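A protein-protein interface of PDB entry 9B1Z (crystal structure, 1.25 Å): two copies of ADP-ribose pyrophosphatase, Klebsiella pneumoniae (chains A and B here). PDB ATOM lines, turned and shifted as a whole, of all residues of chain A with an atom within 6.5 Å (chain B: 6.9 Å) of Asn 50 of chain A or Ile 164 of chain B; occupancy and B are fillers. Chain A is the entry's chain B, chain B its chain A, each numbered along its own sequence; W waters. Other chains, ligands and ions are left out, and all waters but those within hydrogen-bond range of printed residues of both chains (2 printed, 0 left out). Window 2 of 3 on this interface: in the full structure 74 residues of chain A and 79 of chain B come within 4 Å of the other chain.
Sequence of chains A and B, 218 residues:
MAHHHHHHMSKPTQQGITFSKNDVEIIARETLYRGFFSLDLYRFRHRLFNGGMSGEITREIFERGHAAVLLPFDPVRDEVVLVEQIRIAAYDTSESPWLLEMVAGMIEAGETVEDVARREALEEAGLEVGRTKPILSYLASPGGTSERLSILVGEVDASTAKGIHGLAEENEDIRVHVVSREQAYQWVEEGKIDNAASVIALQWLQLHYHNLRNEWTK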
ATOM      1  N   PHE A  19     -32.768   5.127  -9.193  1.00  0.00           N
ATOM      2  CA  PHE A  19     -32.528   6.488  -9.638  1.00  0.00           C
ATOM      3  C   PHE A  19     -32.274   6.529 -11.140  1.00  0.00           C
ATOM      4  O   PHE A  19     -31.846   5.543 -11.754  1.00  0.00           O
ATOM      5  CB  PHE A  19     -31.341   7.058  -8.868  1.00  0.00           C
ATOM      6  CG  PHE A  19     -31.608   7.283  -7.393  1.00  0.00           C
ATOM      7  CD1 PHE A  19     -32.652   8.090  -6.972  1.00  0.00           C
ATOM      8  CD2 PHE A  19     -30.765   6.738  -6.433  1.00  0.00           C
ATOM      9  CE1 PHE A  19     -32.859   8.320  -5.632  1.00  0.00           C
ATOM     10  CE2 PHE A  19     -30.975   6.971  -5.097  1.00  0.00           C
ATOM     11  CZ  PHE A  19     -32.025   7.771  -4.698  1.00  0.00           C
ATOM     12  N   LEU A  48     -28.807  10.447  -2.978  1.00  0.00           N
ATOM     13  CA  LEU A  48     -28.478   9.434  -1.992  1.00  0.00           C
ATOM     14  C   LEU A  48     -29.723   8.631  -1.638  1.00  0.00           C
ATOM     15  O   LEU A  48     -30.834   9.165  -1.603  1.00  0.00           O
ATOM     16  CB  LEU A  48     -27.933  10.100  -0.716  1.00  0.00           C
ATOM     17  CG  LEU A  48     -26.723  11.003  -0.935  1.00  0.00           C
ATOM     18  CD1 LEU A  48     -26.438  11.811   0.316  1.00  0.00           C
ATOM     19  CD2 LEU A  48     -25.525  10.185  -1.343  1.00  0.00           C
ATOM     20  N   PHE A  49     -29.524   7.342  -1.345  1.00  0.00           N
ATOM     21  CA  PHE A  49     -30.648   6.456  -1.037  1.00  0.00           C
ATOM     22  C   PHE A  49     -31.491   6.964   0.121  1.00  0.00           C
ATOM     23  O   PHE A  49     -32.717   6.845   0.084  1.00  0.00           O
ATOM     24  CB  PHE A  49     -30.157   5.031  -0.780  1.00  0.00           C
ATOM     25  CG  PHE A  49     -29.633   4.370  -2.015  1.00  0.00           C
ATOM     26  CD1 PHE A  49     -30.480   4.113  -3.084  1.00  0.00           C
ATOM     27  CD2 PHE A  49     -28.300   4.027  -2.121  1.00  0.00           C
ATOM     28  CE1 PHE A  49     -30.006   3.532  -4.234  1.00  0.00           C
ATOM     29  CE2 PHE A  49     -27.823   3.434  -3.280  1.00  0.00           C
ATOM     30  CZ  PHE A  49     -28.673   3.201  -4.334  1.00  0.00           C
ATOM     31  N   ASN A  50     -30.865   7.525   1.148  1.00  0.00           N
ATOM     32  CA  ASN A  50     -31.604   8.012   2.306  1.00  0.00           C
ATOM     33  C   ASN A  50     -32.037   9.466   2.171  1.00  0.00           C
ATOM     34  O   ASN A  50     -32.495  10.050   3.158  1.00  0.00           O
ATOM     35  CB  ASN A  50     -30.802   7.782   3.596  1.00  0.00           C
ATOM     36  CG  ASN A  50     -30.826   6.330   4.044  1.00  0.00           C
ATOM     37  OD1 ASN A  50     -31.818   5.624   3.846  1.00  0.00           O
ATOM     38  ND2 ASN A  50     -29.738   5.878   4.657  1.00  0.00           N
ATOM     39  N   GLY A  51     -31.926  10.045   0.986  1.00  0.00           N
ATOM     40  CA  GLY A  51     -32.391  11.391   0.723  1.00  0.00           C
ATOM     41  C   GLY A  51     -31.251  12.384   0.616  1.00  0.00           C
ATOM     42  O   GLY A  51     -30.190  12.227   1.228  1.00  0.00           O
ATOM     43  N   GLY A  52     -31.491  13.449  -0.133  1.00  0.00           N
ATOM     44  CA  GLY A  52     -30.482  14.466  -0.337  1.00  0.00           C
ATOM     45  C   GLY A  52     -29.546  14.111  -1.466  1.00  0.00           C
ATOM     46  O   GLY A  52     -29.679  13.086  -2.139  1.00  0.00           O
ATOM     47  N   GLU B 124     -19.691  -4.368   2.033  1.00  0.00           N
ATOM     48  CA  GLU B 124     -20.471  -3.724   0.985  1.00  0.00           C
ATOM     49  C   GLU B 124     -21.959  -4.025   1.103  1.00  0.00           C
ATOM     50  O   GLU B 124     -22.784  -3.217   0.659  1.00  0.00           O
ATOM     51  CB  GLU B 124     -19.943  -4.156  -0.389  1.00  0.00           C
ATOM     52  CG  GLU B 124     -20.602  -3.446  -1.571  1.00  0.00           C
ATOM     53  CD  GLU B 124     -19.852  -3.637  -2.885  1.00  0.00           C
ATOM     54  OE1 GLU B 124     -18.852  -4.396  -2.927  1.00  0.00           O
ATOM     55  OE2 GLU B 124     -20.255  -2.986  -3.878  1.00  0.00           O
ATOM     56  N   LYS B 162     -29.752  -6.266   4.184  1.00  0.00           N
ATOM     57  CA  LYS B 162     -30.592  -5.086   4.346  1.00  0.00           C
ATOM     58  C   LYS B 162     -29.704  -3.867   4.536  1.00  0.00           C
ATOM     59  O   LYS B 162     -28.499  -3.983   4.762  1.00  0.00           O
ATOM     60  CB  LYS B 162     -31.561  -5.251   5.528  1.00  0.00           C
ATOM     61  CG  LYS B 162     -30.898  -5.738   6.813  1.00  0.00           C
ATOM     62  CD  LYS B 162     -31.895  -5.895   7.971  1.00  0.00           C
ATOM     63  CE  LYS B 162     -32.202  -7.356   8.296  1.00  0.00           C
ATOM     64  NZ  LYS B 162     -33.201  -7.502   9.407  1.00  0.00           N
ATOM     65  N   GLY B 163     -30.325  -2.690   4.420  1.00  0.00           N
ATOM     66  CA  GLY B 163     -29.712  -1.447   4.841  1.00  0.00           C
ATOM     67  C   GLY B 163     -28.884  -0.779   3.763  1.00  0.00           C
ATOM     68  O   GLY B 163     -28.670  -1.299   2.661  1.00  0.00           O
ATOM     69  N   ILE B 164     -28.401   0.413   4.107  1.00  0.00           N
ATOM     70  CA  ILE B 164     -27.549   1.216   3.239  1.00  0.00           C
ATOM     71  C   ILE B 164     -26.119   1.094   3.739  1.00  0.00           C
ATOM     72  O   ILE B 164     -25.862   1.141   4.952  1.00  0.00           O
ATOM     73  CB  ILE B 164     -28.022   2.685   3.218  1.00  0.00           C
ATOM     74  CG1 ILE B 164     -29.464   2.769   2.702  1.00  0.00           C
ATOM     75  CG2 ILE B 164     -27.111   3.554   2.337  1.00  0.00           C
ATOM     76  CD1 ILE B 164     -29.661   2.173   1.315  1.00  0.00           C
ATOM     77  N   HIS B 165     -25.187   0.917   2.809  1.00  0.00           N
ATOM     78  CA  HIS B 165     -23.790   0.650   3.121  1.00  0.00           C
ATOM     79  C   HIS B 165     -22.905   1.634   2.376  1.00  0.00           C
ATOM     80  O   HIS B 165     -23.383   2.519   1.659  1.00  0.00           O
ATOM     81  CB  HIS B 165     -23.446  -0.808   2.796  1.00  0.00           C
ATOM     82  CG  HIS B 165     -24.299  -1.775   3.543  1.00  0.00           C
ATOM     83  ND1 HIS B 165     -23.947  -2.271   4.780  1.00  0.00           N
ATOM     84  CD2 HIS B 165     -25.525  -2.280   3.267  1.00  0.00           C
ATOM     85  CE1 HIS B 165     -24.906  -3.066   5.221  1.00  0.00           C
ATOM     86  NE2 HIS B 165     -25.878  -3.082   4.324  1.00  0.00           N
ATOM     87  N   GLY B 166     -21.608   1.485   2.573  1.00  0.00           N
ATOM     88  CA  GLY B 166     -20.629   2.364   1.977  1.00  0.00           C
ATOM     89  C   GLY B 166     -19.919   3.196   3.030  1.00  0.00           C
ATOM     90  O   GLY B 166     -20.471   3.516   4.092  1.00  0.00           O
ATOM     91  N   GLU B 172     -19.239   6.590  -0.755  1.00  0.00           N
ATOM     92  CA  GLU B 172     -19.972   5.425  -1.233  1.00  0.00           C
ATOM     93  C   GLU B 172     -21.370   5.412  -0.630  1.00  0.00           C
ATOM     94  O   GLU B 172     -21.548   5.707   0.554  1.00  0.00           O
ATOM     95  CB  GLU B 172     -19.257   4.129  -0.846  1.00  0.00           C
ATOM     96  CG  GLU B 172     -17.933   3.902  -1.548  1.00  0.00           C
ATOM     97  CD  GLU B 172     -17.296   2.594  -1.139  1.00  0.00           C
ATOM     98  OE1 GLU B 172     -17.504   2.162   0.015  1.00  0.00           O
ATOM     99  OE2 GLU B 172     -16.589   1.996  -1.973  1.00  0.00           O
ATOM    100  N   ASP B 173     -22.358   5.062  -1.455  1.00  0.00           N
ATOM    101  CA  ASP B 173     -23.768   4.997  -1.064  1.00  0.00           C
ATOM    102  C   ASP B 173     -24.352   3.774  -1.767  1.00  0.00           C
ATOM    103  O   ASP B 173     -24.451   3.754  -2.993  1.00  0.00           O
ATOM    104  CB  ASP B 173     -24.474   6.289  -1.489  1.00  0.00           C
ATOM    105  CG  ASP B 173     -25.898   6.385  -0.977  1.00  0.00           C
ATOM    106  OD1 ASP B 173     -26.116   6.155   0.230  1.00  0.00           O
ATOM    107  OD2 ASP B 173     -26.800   6.702  -1.784  1.00  0.00           O
ATOM    108  N   ILE B 174     -24.697   2.740  -1.009  1.00  0.00           N
ATOM    109  CA  ILE B 174     -24.974   1.418  -1.559  1.00  0.00           C
ATOM    110  C   ILE B 174     -26.282   0.893  -0.967  1.00  0.00           C
ATOM    111  O   ILE B 174     -26.473   0.940   0.249  1.00  0.00           O
ATOM    112  CB  ILE B 174     -23.803   0.450  -1.275  1.00  0.00           C
ATOM    113  CG1 ILE B 174     -22.474   1.072  -1.736  1.00  0.00           C
ATOM    114  CG2 ILE B 174     -24.045  -0.883  -1.950  1.00  0.00           C
ATOM    115  CD1 ILE B 174     -21.234   0.262  -1.356  1.00  0.00           C
ATOM    116  N   ARG B 175     -27.171   0.385  -1.832  1.00  0.00           N
ATOM    117  CA  ARG B 175     -28.434  -0.241  -1.436  1.00  0.00           C
ATOM    118  C   ARG B 175     -28.394  -1.725  -1.766  1.00  0.00           C
ATOM    119  O   ARG B 175     -27.879  -2.122  -2.811  1.00  0.00           O
ATOM    120  CB  ARG B 175     -29.624   0.408  -2.184  1.00  0.00           C
ATOM    121  CG  ARG B 175     -30.978  -0.274  -2.032  1.00  0.00           C
ATOM    122  CD  ARG B 175     -32.074   0.585  -2.593  1.00  0.00           C
ATOM    123  NE  ARG B 175     -32.571   1.506  -1.580  1.00  0.00           N
ATOM    124  CZ  ARG B 175     -33.512   2.414  -1.793  1.00  0.00           C
ATOM    125  NH1 ARG B 175     -34.055   2.576  -2.989  1.00  0.00           N
ATOM    126  NH2 ARG B 175     -33.910   3.184  -0.784  1.00  0.00           N
ATOM    127  N   VAL B 176     -28.973  -2.544  -0.926  1.00  0.00           N
ATOM    128  CA  VAL B 176     -29.030  -3.982  -1.141  1.00  0.00           C
ATOM    129  C   VAL B 176     -30.388  -4.358  -1.716  1.00  0.00           C
ATOM    130  O   VAL B 176     -31.422  -3.852  -1.266  1.00  0.00           O
ATOM    131  CB  VAL B 176     -28.787  -4.708   0.194  1.00  0.00           C
ATOM    132  CG1 VAL B 176     -29.029  -6.190   0.053  1.00  0.00           C
ATOM    133  CG2 VAL B 176     -27.372  -4.432   0.695  1.00  0.00           C
HETATM  134  O   HOH W   1     -28.048   7.302   1.686  1.00  0.00           O
HETATM  135  O   HOH W   2     -34.479   5.647  -2.102  1.00  0.00           O
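Water W1 lies within hydrogen-bond range of the side-chain carboxylate (OD1) of Asp 173 of chain B (2.7 Å), the backbone NH (N) of Asn 50 of chain A (2.9 Å) and the backbone NH (N) of Phe 49 of chain A (3.4 Å).
Water W2 bridges NH2 of Arg 175 of chain B (2.9 Å) and O of Phe 49 of chain A (3.1 Å).
OD2 of Asp 173 of chain B touches CA of Leu 48 of chain A (3.2 Å).
Ile 164 of chain B touches Phe 49 of chain A.
C of Ile 174 of chain B touches CE2 of Phe 49 of chain A (3.8 Å).
Arg 175 of chain B touches Phe 49 of chain A.
Asn 50 of chain A touches Ile 164 of chain B (ND2 to CG1, 3.7 Å).
The side-chain carboxylate (OD2) of Asp 173 of chain B sits at hydrogen-bond distance from the backbone NH (N) of Phe 49 of chain A (2.8 Å).
Hydrophobic or aromatic side chains of chain A that line the printed part of chain B: Leu 48 and Phe 49.
Hydrophobic or aromatic side chains of chain B within 4 Å of the printed part of chain A: Ile 164.
Printed residues of chain B within 4 Å of Leu 48 of chain A: Asp 173 (3.2 Å).
Asn 50 of chain A touches one residue of chain B.
Lys 162 of chain B touches none of the printed residues of chain A.
Printed residues of chain A within 4 Å of Arg 175 of chain B: Phe 49 (3.4 Å).
The nearest printed residue of chain B that does not touch Leu 48 of chain A is Glu 172 of chain B (6.3 Å).
N of His 165 of chain B sits at hydrogen-bond distance from O of Ile 174 of chain B (2.9 Å).
No position is printed for both chains.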
